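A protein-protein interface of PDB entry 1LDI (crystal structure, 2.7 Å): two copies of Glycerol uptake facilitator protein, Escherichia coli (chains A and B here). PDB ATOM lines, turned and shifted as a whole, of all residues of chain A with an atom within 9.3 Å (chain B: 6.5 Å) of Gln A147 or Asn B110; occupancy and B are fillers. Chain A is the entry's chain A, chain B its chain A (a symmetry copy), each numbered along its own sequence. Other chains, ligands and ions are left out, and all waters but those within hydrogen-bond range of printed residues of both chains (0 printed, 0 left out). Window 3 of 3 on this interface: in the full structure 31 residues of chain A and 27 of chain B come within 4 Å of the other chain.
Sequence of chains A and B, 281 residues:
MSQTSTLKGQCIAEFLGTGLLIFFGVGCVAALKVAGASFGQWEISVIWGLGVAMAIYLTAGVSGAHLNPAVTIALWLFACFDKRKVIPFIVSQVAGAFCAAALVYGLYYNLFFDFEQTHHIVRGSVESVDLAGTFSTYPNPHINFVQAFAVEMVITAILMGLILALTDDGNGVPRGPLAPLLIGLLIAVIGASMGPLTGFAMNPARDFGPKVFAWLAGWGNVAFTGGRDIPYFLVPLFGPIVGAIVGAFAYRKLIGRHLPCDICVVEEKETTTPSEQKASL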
ATOM      1  N   PRO A 139      21.641 -14.578  27.556  1.00  0.00           N
ATOM      2  CA  PRO A 139      20.748 -15.437  26.772  1.00  0.00           C
ATOM      3  C   PRO A 139      20.581 -16.859  27.317  1.00  0.00           C
ATOM      4  O   PRO A 139      21.542 -17.466  27.786  1.00  0.00           O
ATOM      5  CB  PRO A 139      21.411 -15.434  25.409  1.00  0.00           C
ATOM      6  CG  PRO A 139      22.858 -15.510  25.791  1.00  0.00           C
ATOM      7  CD  PRO A 139      22.957 -14.474  26.902  1.00  0.00           C
ATOM      8  N   ASN A 140      19.360 -17.382  27.247  1.00  0.00           N
ATOM      9  CA  ASN A 140      19.082 -18.736  27.704  1.00  0.00           C
ATOM     10  C   ASN A 140      20.014 -19.672  26.930  1.00  0.00           C
ATOM     11  O   ASN A 140      20.289 -19.443  25.755  1.00  0.00           O
ATOM     12  CB  ASN A 140      17.612 -19.070  27.422  1.00  0.00           C
ATOM     13  CG  ASN A 140      17.238 -20.494  27.808  1.00  0.00           C
ATOM     14  OD1 ASN A 140      17.696 -21.459  27.190  1.00  0.00           O
ATOM     15  ND2 ASN A 140      16.395 -20.628  28.830  1.00  0.00           N
ATOM     16  N   PRO A 141      20.516 -20.733  27.575  1.00  0.00           N
ATOM     17  CA  PRO A 141      21.424 -21.686  26.925  1.00  0.00           C
ATOM     18  C   PRO A 141      20.997 -22.231  25.558  1.00  0.00           C
ATOM     19  O   PRO A 141      21.840 -22.444  24.687  1.00  0.00           O
ATOM     20  CB  PRO A 141      21.551 -22.795  27.959  1.00  0.00           C
ATOM     21  CG  PRO A 141      21.461 -22.055  29.231  1.00  0.00           C
ATOM     22  CD  PRO A 141      20.302 -21.106  28.980  1.00  0.00           C
ATOM     23  N   HIS A 142      19.698 -22.448  25.370  1.00  0.00           N
ATOM     24  CA  HIS A 142      19.174 -22.999  24.119  1.00  0.00           C
ATOM     25  C   HIS A 142      18.967 -22.047  22.937  1.00  0.00           C
ATOM     26  O   HIS A 142      18.483 -22.472  21.887  1.00  0.00           O
ATOM     27  CB  HIS A 142      17.858 -23.725  24.393  1.00  0.00           C
ATOM     28  CG  HIS A 142      17.951 -24.749  25.476  1.00  0.00           C
ATOM     29  ND1 HIS A 142      17.929 -24.419  26.814  1.00  0.00           N
ATOM     30  CD2 HIS A 142      18.082 -26.097  25.421  1.00  0.00           C
ATOM     31  CE1 HIS A 142      18.039 -25.521  27.538  1.00  0.00           C
ATOM     32  NE2 HIS A 142      18.133 -26.552  26.717  1.00  0.00           N
ATOM     33  N   ILE A 143      19.322 -20.773  23.083  1.00  0.00           N
ATOM     34  CA  ILE A 143      19.141 -19.845  21.971  1.00  0.00           C
ATOM     35  C   ILE A 143      20.409 -19.060  21.645  1.00  0.00           C
ATOM     36  O   ILE A 143      21.267 -18.869  22.503  1.00  0.00           O
ATOM     37  CB  ILE A 143      17.973 -18.859  22.229  1.00  0.00           C
ATOM     38  CG1 ILE A 143      18.356 -17.830  23.293  1.00  0.00           C
ATOM     39  CG2 ILE A 143      16.723 -19.641  22.655  1.00  0.00           C
ATOM     40  CD1 ILE A 143      17.281 -16.792  23.518  1.00  0.00           C
ATOM     41  N   ASN A 144      20.518 -18.611  20.397  1.00  0.00           N
ATOM     42  CA  ASN A 144      21.692 -17.874  19.936  1.00  0.00           C
ATOM     43  C   ASN A 144      21.515 -16.359  19.924  1.00  0.00           C
ATOM     44  O   ASN A 144      20.500 -15.828  20.364  1.00  0.00           O
ATOM     45  CB  ASN A 144      22.072 -18.337  18.527  1.00  0.00           C
ATOM     46  CG  ASN A 144      20.934 -18.164  17.530  1.00  0.00           C
ATOM     47  OD1 ASN A 144      20.123 -17.243  17.647  1.00  0.00           O
ATOM     48  ND2 ASN A 144      20.880 -19.038  16.535  1.00  0.00           N
ATOM     49  N   PHE A 145      22.521 -15.677  19.390  1.00  0.00           N
ATOM     50  CA  PHE A 145      22.535 -14.224  19.290  1.00  0.00           C
ATOM     51  C   PHE A 145      21.309 -13.645  18.577  1.00  0.00           C
ATOM     52  O   PHE A 145      20.648 -12.759  19.106  1.00  0.00           O
ATOM     53  CB  PHE A 145      23.797 -13.788  18.555  1.00  0.00           C
ATOM     54  CG  PHE A 145      24.029 -12.306  18.563  1.00  0.00           C
ATOM     55  CD1 PHE A 145      24.665 -11.693  19.640  1.00  0.00           C
ATOM     56  CD2 PHE A 145      23.639 -11.520  17.481  1.00  0.00           C
ATOM     57  CE1 PHE A 145      24.918 -10.316  19.641  1.00  0.00           C
ATOM     58  CE2 PHE A 145      23.883 -10.141  17.471  1.00  0.00           C
ATOM     59  CZ  PHE A 145      24.526  -9.540  18.554  1.00  0.00           C
ATOM     60  N   VAL A 146      21.009 -14.140  17.378  1.00  0.00           N
ATOM     61  CA  VAL A 146      19.874 -13.637  16.606  1.00  0.00           C
ATOM     62  C   VAL A 146      18.512 -13.933  17.229  1.00  0.00           C
ATOM     63  O   VAL A 146      17.613 -13.084  17.195  1.00  0.00           O
ATOM     64  CB  VAL A 146      19.899 -14.182  15.167  1.00  0.00           C
ATOM     65  CG1 VAL A 146      18.675 -13.710  14.413  1.00  0.00           C
ATOM     66  CG2 VAL A 146      21.153 -13.697  14.460  1.00  0.00           C
ATOM     67  N   GLN A 147      18.356 -15.133  17.787  1.00  0.00           N
ATOM     68  CA  GLN A 147      17.106 -15.513  18.439  1.00  0.00           C
ATOM     69  C   GLN A 147      16.905 -14.569  19.618  1.00  0.00           C
ATOM     70  O   GLN A 147      15.805 -14.072  19.852  1.00  0.00           O
ATOM     71  CB  GLN A 147      17.182 -16.951  18.957  1.00  0.00           C
ATOM     72  CG  GLN A 147      16.882 -18.029  17.936  1.00  0.00           C
ATOM     73  CD  GLN A 147      17.820 -19.237  18.048  1.00  0.00           C
ATOM     74  OE1 GLN A 147      18.215 -19.650  19.146  1.00  0.00           O
ATOM     75  NE2 GLN A 147      18.169 -19.811  16.903  1.00  0.00           N
ATOM     76  N   ALA A 148      17.986 -14.325  20.355  1.00  0.00           N
ATOM     77  CA  ALA A 148      17.955 -13.450  21.513  1.00  0.00           C
ATOM     78  C   ALA A 148      17.623 -12.022  21.104  1.00  0.00           C
ATOM     79  O   ALA A 148      16.947 -11.305  21.837  1.00  0.00           O
ATOM     80  CB  ALA A 148      19.290 -13.494  22.235  1.00  0.00           C
ATOM     81  N   PHE A 149      18.095 -11.613  19.931  1.00  0.00           N
ATOM     82  CA  PHE A 149      17.839 -10.261  19.443  1.00  0.00           C
ATOM     83  C   PHE A 149      16.352 -10.099  19.130  1.00  0.00           C
ATOM     84  O   PHE A 149      15.765  -9.049  19.394  1.00  0.00           O
ATOM     85  CB  PHE A 149      18.658  -9.982  18.182  1.00  0.00           C
ATOM     86  CG  PHE A 149      18.582  -8.549  17.709  1.00  0.00           C
ATOM     87  CD1 PHE A 149      19.541  -7.619  18.101  1.00  0.00           C
ATOM     88  CD2 PHE A 149      17.557  -8.131  16.855  1.00  0.00           C
ATOM     89  CE1 PHE A 149      19.485  -6.296  17.644  1.00  0.00           C
ATOM     90  CE2 PHE A 149      17.495  -6.804  16.393  1.00  0.00           C
ATOM     91  CZ  PHE A 149      18.458  -5.892  16.788  1.00  0.00           C
ATOM     92  N   ALA A 150      15.758 -11.145  18.560  1.00  0.00           N
ATOM     93  CA  ALA A 150      14.349 -11.143  18.212  1.00  0.00           C
ATOM     94  C   ALA A 150      13.513 -10.922  19.465  1.00  0.00           C
ATOM     95  O   ALA A 150      12.598 -10.093  19.472  1.00  0.00           O
ATOM     96  CB  ALA A 150      13.977 -12.460  17.561  1.00  0.00           C
ATOM     97  N   VAL A 151      13.836 -11.661  20.527  1.00  0.00           N
ATOM     98  CA  VAL A 151      13.119 -11.564  21.798  1.00  0.00           C
ATOM     99  C   VAL A 151      13.097 -10.149  22.378  1.00  0.00           C
ATOM    100  O   VAL A 151      12.026  -9.604  22.670  1.00  0.00           O
ATOM    101  CB  VAL A 151      13.730 -12.490  22.875  1.00  0.00           C
ATOM    102  CG1 VAL A 151      12.939 -12.357  24.178  1.00  0.00           C
ATOM    103  CG2 VAL A 151      13.739 -13.928  22.396  1.00  0.00           C
ATOM    104  N   GLU A 152      14.277  -9.565  22.569  1.00  0.00           N
ATOM    105  CA  GLU A 152      14.357  -8.220  23.131  1.00  0.00           C
ATOM    106  C   GLU A 152      13.613  -7.232  22.247  1.00  0.00           C
ATOM    107  O   GLU A 152      12.933  -6.321  22.732  1.00  0.00           O
ATOM    108  CB  GLU A 152      15.822  -7.787  23.286  1.00  0.00           C
ATOM    109  CG  GLU A 152      16.559  -8.483  24.430  1.00  0.00           C
ATOM    110  CD  GLU A 152      16.046  -8.064  25.795  1.00  0.00           C
ATOM    111  OE1 GLU A 152      16.353  -8.755  26.783  1.00  0.00           O
ATOM    112  OE2 GLU A 152      15.340  -7.037  25.886  1.00  0.00           O
ATOM    113  N   MET A 153      13.732  -7.437  20.943  1.00  0.00           N
ATOM    114  CA  MET A 153      13.088  -6.574  19.977  1.00  0.00           C
ATOM    115  C   MET A 153      11.569  -6.613  20.129  1.00  0.00           C
ATOM    116  O   MET A 153      10.931  -5.587  20.333  1.00  0.00           O
ATOM    117  CB  MET A 153      13.492  -6.998  18.566  1.00  0.00           C
ATOM    118  CG  MET A 153      13.117  -5.997  17.494  1.00  0.00           C
ATOM    119  SD  MET A 153      13.781  -6.473  15.905  1.00  0.00           S
ATOM    120  CE  MET A 153      12.376  -7.392  15.228  1.00  0.00           C
ATOM    121  N   VAL A 154      10.995  -7.804  20.040  1.00  0.00           N
ATOM    122  CA  VAL A 154       9.552  -7.959  20.155  1.00  0.00           C
ATOM    123  C   VAL A 154       9.004  -7.401  21.453  1.00  0.00           C
ATOM    124  O   VAL A 154       8.111  -6.551  21.442  1.00  0.00           O
ATOM    125  CB  VAL A 154       9.134  -9.449  20.055  1.00  0.00           C
ATOM    126  CG1 VAL A 154       7.639  -9.594  20.313  1.00  0.00           C
ATOM    127  CG2 VAL A 154       9.492 -10.000  18.682  1.00  0.00           C
ATOM    128  N   ILE A 155       9.542  -7.877  22.571  1.00  0.00           N
ATOM    129  CA  ILE A 155       9.071  -7.442  23.879  1.00  0.00           C
ATOM    130  C   ILE A 155       9.181  -5.945  24.143  1.00  0.00           C
ATOM    131  O   ILE A 155       8.277  -5.366  24.743  1.00  0.00           O
ATOM    132  CB  ILE A 155       9.781  -8.195  25.023  1.00  0.00           C
ATOM    133  CG1 ILE A 155      11.264  -7.854  25.040  1.00  0.00           C
ATOM    134  CG2 ILE A 155       9.588  -9.684  24.853  1.00  0.00           C
ATOM    135  CD1 ILE A 155      11.962  -8.309  26.309  1.00  0.00           C
ATOM    136  N   MET A 194       8.161 -13.853  28.977  1.00  0.00           N
ATOM    137  CA  MET A 194       9.327 -13.891  28.095  1.00  0.00           C
ATOM    138  C   MET A 194      10.672 -13.847  28.813  1.00  0.00           C
ATOM    139  O   MET A 194      11.720 -14.023  28.190  1.00  0.00           O
ATOM    140  CB  MET A 194       9.261 -12.725  27.103  1.00  0.00           C
ATOM    141  CG  MET A 194       8.183 -12.860  26.039  1.00  0.00           C
ATOM    142  SD  MET A 194       8.406 -14.340  25.024  1.00  0.00           S
ATOM    143  CE  MET A 194       6.802 -15.109  25.141  1.00  0.00           C
ATOM    144  N   LEU A 197      13.938 -16.286  28.507  1.00  0.00           N
ATOM    145  CA  LEU A 197      14.683 -16.300  27.253  1.00  0.00           C
ATOM    146  C   LEU A 197      15.915 -15.394  27.259  1.00  0.00           C
ATOM    147  O   LEU A 197      17.020 -15.844  26.928  1.00  0.00           O
ATOM    148  CB  LEU A 197      13.766 -15.927  26.092  1.00  0.00           C
ATOM    149  CG  LEU A 197      12.731 -16.974  25.677  1.00  0.00           C
ATOM    150  CD1 LEU A 197      11.877 -16.393  24.553  1.00  0.00           C
ATOM    151  CD2 LEU A 197      13.410 -18.268  25.226  1.00  0.00           C
ATOM    152  N   THR A 198      15.737 -14.126  27.638  1.00  0.00           N
ATOM    153  CA  THR A 198      16.859 -13.191  27.666  1.00  0.00           C
ATOM    154  C   THR A 198      16.908 -12.262  28.886  1.00  0.00           C
ATOM    155  O   THR A 198      17.662 -11.289  28.898  1.00  0.00           O
ATOM    156  CB  THR A 198      16.882 -12.314  26.390  1.00  0.00           C
ATOM    157  OG1 THR A 198      15.748 -11.440  26.385  1.00  0.00           O
ATOM    158  CG2 THR A 198      16.835 -13.176  25.149  1.00  0.00           C
ATOM    159  N   ARG A 228      30.106 -16.424  25.125  1.00  0.00           N
ATOM    160  CA  ARG A 228      29.644 -16.821  23.792  1.00  0.00           C
ATOM    161  C   ARG A 228      30.545 -16.235  22.685  1.00  0.00           C
ATOM    162  O   ARG A 228      31.417 -15.408  22.959  1.00  0.00           O
ATOM    163  CB  ARG A 228      28.202 -16.346  23.604  1.00  0.00           C
ATOM    164  CG  ARG A 228      27.344 -16.451  24.869  1.00  0.00           C
ATOM    165  CD  ARG A 228      26.619 -17.784  25.010  1.00  0.00           C
ATOM    166  NE  ARG A 228      25.634 -17.966  23.946  1.00  0.00           N
ATOM    167  CZ  ARG A 228      24.419 -18.493  24.104  1.00  0.00           C
ATOM    168  NH1 ARG A 228      23.997 -18.907  25.290  1.00  0.00           N
ATOM    169  NH2 ARG A 228      23.618 -18.605  23.059  1.00  0.00           N
ATOM    170  N   ILE A 230      29.630 -14.349  19.846  1.00  0.00           N
ATOM    171  CA  ILE A 230      29.304 -12.966  19.524  1.00  0.00           C
ATOM    172  C   ILE A 230      29.057 -12.265  20.859  1.00  0.00           C
ATOM    173  O   ILE A 230      28.289 -12.753  21.684  1.00  0.00           O
ATOM    174  CB  ILE A 230      28.045 -12.877  18.646  1.00  0.00           C
ATOM    175  CG1 ILE A 230      28.205 -13.787  17.422  1.00  0.00           C
ATOM    176  CG2 ILE A 230      27.830 -11.434  18.195  1.00  0.00           C
ATOM    177  CD1 ILE A 230      26.983 -13.855  16.527  1.00  0.00           C
ATOM    178  N   TYR A 232      27.546 -10.712  23.647  1.00  0.00           N
ATOM    179  CA  TYR A 232      26.130 -10.559  23.957  1.00  0.00           C
ATOM    180  C   TYR A 232      25.590  -9.159  24.285  1.00  0.00           C
ATOM    181  O   TYR A 232      24.427  -8.862  24.006  1.00  0.00           O
ATOM    182  CB  TYR A 232      25.739 -11.520  25.085  1.00  0.00           C
ATOM    183  CG  TYR A 232      24.247 -11.603  25.266  1.00  0.00           C
ATOM    184  CD1 TYR A 232      23.441 -12.201  24.294  1.00  0.00           C
ATOM    185  CD2 TYR A 232      23.625 -11.024  26.369  1.00  0.00           C
ATOM    186  CE1 TYR A 232      22.046 -12.213  24.416  1.00  0.00           C
ATOM    187  CE2 TYR A 232      22.235 -11.027  26.498  1.00  0.00           C
ATOM    188  CZ  TYR A 232      21.451 -11.620  25.522  1.00  0.00           C
ATOM    189  OH  TYR A 232      20.081 -11.608  25.646  1.00  0.00           O
ATOM    190  N   VAL A 235      22.979  -7.208  22.077  1.00  0.00           N
ATOM    191  CA  VAL A 235      21.540  -7.474  22.026  1.00  0.00           C
ATOM    192  C   VAL A 235      20.719  -6.565  22.953  1.00  0.00           C
ATOM    193  O   VAL A 235      19.748  -5.947  22.519  1.00  0.00           O
ATOM    194  CB  VAL A 235      21.214  -8.951  22.374  1.00  0.00           C
ATOM    195  CG1 VAL A 235      19.721  -9.206  22.208  1.00  0.00           C
ATOM    196  CG2 VAL A 235      22.005  -9.891  21.481  1.00  0.00           C
ATOM    197  N   TYR B 105       5.433 -19.520  20.455  1.00  0.00           N
ATOM    198  CA  TYR B 105       6.153 -20.726  20.065  1.00  0.00           C
ATOM    199  C   TYR B 105       7.441 -20.309  19.355  1.00  0.00           C
ATOM    200  O   TYR B 105       8.498 -20.917  19.543  1.00  0.00           O
ATOM    201  CB  TYR B 105       5.297 -21.562  19.114  1.00  0.00           C
ATOM    202  CG  TYR B 105       5.979 -22.805  18.594  1.00  0.00           C
ATOM    203  CD1 TYR B 105       6.252 -23.883  19.436  1.00  0.00           C
ATOM    204  CD2 TYR B 105       6.344 -22.908  17.253  1.00  0.00           C
ATOM    205  CE1 TYR B 105       6.875 -25.045  18.948  1.00  0.00           C
ATOM    206  CE2 TYR B 105       6.965 -24.053  16.752  1.00  0.00           C
ATOM    207  CZ  TYR B 105       7.230 -25.120  17.601  1.00  0.00           C
ATOM    208  OH  TYR B 105       7.856 -26.244  17.108  1.00  0.00           O
ATOM    209  N   GLY B 106       7.346 -19.269  18.532  1.00  0.00           N
ATOM    210  CA  GLY B 106       8.515 -18.799  17.820  1.00  0.00           C
ATOM    211  C   GLY B 106       9.642 -18.466  18.778  1.00  0.00           C
ATOM    212  O   GLY B 106      10.777 -18.913  18.588  1.00  0.00           O
ATOM    213  N   LEU B 107       9.326 -17.703  19.823  1.00  0.00           N
ATOM    214  CA  LEU B 107      10.323 -17.279  20.806  1.00  0.00           C
ATOM    215  C   LEU B 107      10.844 -18.385  21.716  1.00  0.00           C
ATOM    216  O   LEU B 107      11.989 -18.334  22.157  1.00  0.00           O
ATOM    217  CB  LEU B 107       9.750 -16.152  21.662  1.00  0.00           C
ATOM    218  CG  LEU B 107       9.315 -14.903  20.897  1.00  0.00           C
ATOM    219  CD1 LEU B 107       8.515 -13.992  21.810  1.00  0.00           C
ATOM    220  CD2 LEU B 107      10.535 -14.177  20.355  1.00  0.00           C
ATOM    221  N   TYR B 108       9.998 -19.376  21.993  1.00  0.00           N
ATOM    222  CA  TYR B 108      10.352 -20.505  22.856  1.00  0.00           C
ATOM    223  C   TYR B 108      10.727 -21.762  22.062  1.00  0.00           C
ATOM    224  O   TYR B 108      11.002 -22.807  22.656  1.00  0.00           O
ATOM    225  CB  TYR B 108       9.176 -20.862  23.780  1.00  0.00           C
ATOM    226  CG  TYR B 108       9.073 -20.058  25.064  1.00  0.00           C
ATOM    227  CD1 TYR B 108       8.448 -18.807  25.093  1.00  0.00           C
ATOM    228  CD2 TYR B 108       9.588 -20.559  26.261  1.00  0.00           C
ATOM    229  CE1 TYR B 108       8.338 -18.085  26.287  1.00  0.00           C
ATOM    230  CE2 TYR B 108       9.482 -19.844  27.451  1.00  0.00           C
ATOM    231  CZ  TYR B 108       8.858 -18.613  27.463  1.00  0.00           C
ATOM    232  OH  TYR B 108       8.748 -17.921  28.652  1.00  0.00           O
ATOM    233  N   TYR B 109      10.706 -21.661  20.731  1.00  0.00           N
ATOM    234  CA  TYR B 109      11.015 -22.772  19.815  1.00  0.00           C
ATOM    235  C   TYR B 109      12.013 -23.815  20.345  1.00  0.00           C
ATOM    236  O   TYR B 109      11.695 -24.998  20.457  1.00  0.00           O
ATOM    237  CB  TYR B 109      11.559 -22.199  18.505  1.00  0.00           C
ATOM    238  CG  TYR B 109      11.816 -23.213  17.419  1.00  0.00           C
ATOM    239  CD1 TYR B 109      10.782 -23.649  16.593  1.00  0.00           C
ATOM    240  CD2 TYR B 109      13.096 -23.722  17.198  1.00  0.00           C
ATOM    241  CE1 TYR B 109      11.010 -24.565  15.561  1.00  0.00           C
ATOM    242  CE2 TYR B 109      13.342 -24.646  16.174  1.00  0.00           C
ATOM    243  CZ  TYR B 109      12.290 -25.064  15.351  1.00  0.00           C
ATOM    244  OH  TYR B 109      12.512 -25.955  14.314  1.00  0.00           O
ATOM    245  N   ASN B 110      13.223 -23.365  20.659  1.00  0.00           N
ATOM    246  CA  ASN B 110      14.276 -24.246  21.140  1.00  0.00           C
ATOM    247  C   ASN B 110      13.939 -25.009  22.401  1.00  0.00           C
ATOM    248  O   ASN B 110      14.209 -26.205  22.503  1.00  0.00           O
ATOM    249  CB  ASN B 110      15.546 -23.444  21.378  1.00  0.00           C
ATOM    250  CG  ASN B 110      16.067 -22.812  20.121  1.00  0.00           C
ATOM    251  OD1 ASN B 110      16.624 -23.493  19.265  1.00  0.00           O
ATOM    252  ND2 ASN B 110      15.879 -21.494  19.991  1.00  0.00           N
ATOM    253  N   LEU B 111      13.370 -24.316  23.375  1.00  0.00           N
ATOM    254  CA  LEU B 111      13.030 -24.965  24.625  1.00  0.00           C
ATOM    255  C   LEU B 111      12.056 -26.114  24.421  1.00  0.00           C
ATOM    256  O   LEU B 111      12.129 -27.127  25.124  1.00  0.00           O
ATOM    257  CB  LEU B 111      12.473 -23.950  25.617  1.00  0.00           C
ATOM    258  CG  LEU B 111      13.566 -23.081  26.242  1.00  0.00           C
ATOM    259  CD1 LEU B 111      13.940 -21.941  25.298  1.00  0.00           C
ATOM    260  CD2 LEU B 111      13.068 -22.536  27.566  1.00  0.00           C
ATOM    261  N   PHE B 112      11.153 -25.974  23.455  1.00  0.00           N
ATOM    262  CA  PHE B 112      10.195 -27.035  23.184  1.00  0.00           C
ATOM    263  C   PHE B 112      10.901 -28.287  22.697  1.00  0.00           C
ATOM    264  O   PHE B 112      10.658 -29.379  23.213  1.00  0.00           O
ATOM    265  CB  PHE B 112       9.163 -26.600  22.146  1.00  0.00           C
ATOM    266  CG  PHE B 112       7.978 -25.888  22.733  1.00  0.00           C
ATOM    267  CD1 PHE B 112       7.872 -24.504  22.659  1.00  0.00           C
ATOM    268  CD2 PHE B 112       6.966 -26.603  23.374  1.00  0.00           C
ATOM    269  CE1 PHE B 112       6.768 -23.840  23.214  1.00  0.00           C
ATOM    270  CE2 PHE B 112       5.866 -25.950  23.930  1.00  0.00           C
ATOM    271  CZ  PHE B 112       5.768 -24.565  23.849  1.00  0.00           C
ATOM    272  N   PHE B 113      11.786 -28.133  21.717  1.00  0.00           N
ATOM    273  CA  PHE B 113      12.497 -29.281  21.178  1.00  0.00           C
ATOM    274  C   PHE B 113      13.501 -29.893  22.132  1.00  0.00           C
ATOM    275  O   PHE B 113      13.555 -31.112  22.267  1.00  0.00           O
ATOM    276  CB  PHE B 113      13.176 -28.917  19.860  1.00  0.00           C
ATOM    277  CG  PHE B 113      12.201 -28.655  18.745  1.00  0.00           C
ATOM    278  CD1 PHE B 113      11.537 -27.426  18.652  1.00  0.00           C
ATOM    279  CD2 PHE B 113      11.886 -29.659  17.832  1.00  0.00           C
ATOM    280  CE1 PHE B 113      10.575 -27.203  17.674  1.00  0.00           C
ATOM    281  CE2 PHE B 113      10.922 -29.447  16.848  1.00  0.00           C
ATOM    282  CZ  PHE B 113      10.266 -28.217  16.770  1.00  0.00           C
ATOM    283  N   ASP B 114      14.295 -29.057  22.793  1.00  0.00           N
ATOM    284  CA  ASP B 114      15.287 -29.546  23.743  1.00  0.00           C
ATOM    285  C   ASP B 114      14.609 -30.273  24.892  1.00  0.00           C
ATOM    286  O   ASP B 114      15.143 -31.247  25.410  1.00  0.00           O
ATOM    287  CB  ASP B 114      16.125 -28.385  24.282  1.00  0.00           C
ATOM    288  CG  ASP B 114      16.896 -27.662  23.182  1.00  0.00           C
ATOM    289  OD1 ASP B 114      17.719 -28.310  22.499  1.00  0.00           O
ATOM    290  OD2 ASP B 114      16.680 -26.444  22.995  1.00  0.00           O
ATOM    291  N   PHE B 115      13.426 -29.807  25.286  1.00  0.00           N
ATOM    292  CA  PHE B 115      12.698 -30.443  26.380  1.00  0.00           C
ATOM    293  C   PHE B 115      12.165 -31.802  25.963  1.00  0.00           C
ATOM    294  O   PHE B 115      12.267 -32.767  26.718  1.00  0.00           O
ATOM    295  CB  PHE B 115      11.518 -29.584  26.834  1.00  0.00           C
ATOM    296  CG  PHE B 115      10.823 -30.116  28.059  1.00  0.00           C
ATOM    297  CD1 PHE B 115      11.184 -29.676  29.325  1.00  0.00           C
ATOM    298  CD2 PHE B 115       9.814 -31.066  27.947  1.00  0.00           C
ATOM    299  CE1 PHE B 115      10.554 -30.172  30.464  1.00  0.00           C
ATOM    300  CE2 PHE B 115       9.177 -31.570  29.085  1.00  0.00           C
ATOM    301  CZ  PHE B 115       9.553 -31.117  30.345  1.00  0.00           C
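The side-chain amide nitrogen (ND2) of Asn B110 sits close to the backbone carbonyl oxygen (O) of His A142 (3.4 Å). The side-chain amide oxygen (OE1) of Gln A147 lies within hydrogen-bond range of the side-chain amide nitrogen (ND2) of Asn B110, at 3.1 Å.
OD1 of Asn A140 lies within hydrogen-bond range of N of His A142. O of Leu A197 sits at hydrogen-bond distance from N of Asn A140, 2.8 Å away. The backbone carbonyl oxygen (O) of Ile A143 is in hydrogen-bond range of the guanidinium group (NH2) of Arg A228 (2.4 Å). OD1 of Asn A144 lies within hydrogen-bond range of N of Gln A147, at 2.8 Å. O of Asn B110 lies close to OD2 of Asp B114 (2.5 Å).
His A142 touches Asp B114 (CD2 to OD2, 2.8 Å). Asn B110 touches Ile A143 (ND2 to CG2, 3.4 Å). Val A151 touches Leu B107 (CG2 to CD2, 3.8 Å). Met A194 touches Leu B107. Tyr B108 touches Met A194. Leu B107 touches Leu A197. Leu B111 touches Leu A197 (CD1 to CD2, 3.7 Å).
Gln A147 touches one residue of chain B. Asn B110 touches three residues of chain A. Printed residues of chain A within 4 Å of Leu B111: Leu A197. Printed residues of chain A within 4 Å of Tyr B108: Met A194 (3.5 Å). Glu A152 touches none of the printed residues of chain B. The nearest printed residue of chain B that does not touch Ile A143 is Leu B111 (4.5 Å).
Hydrophobic or aromatic side chains of chain B within 4 Å of the printed part of chain A: Leu B107, Tyr B108 and Leu B111. Along chain A the printed residues that touch a printed residue of chain B span positions 142 to 197.
No position is printed for both chains.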
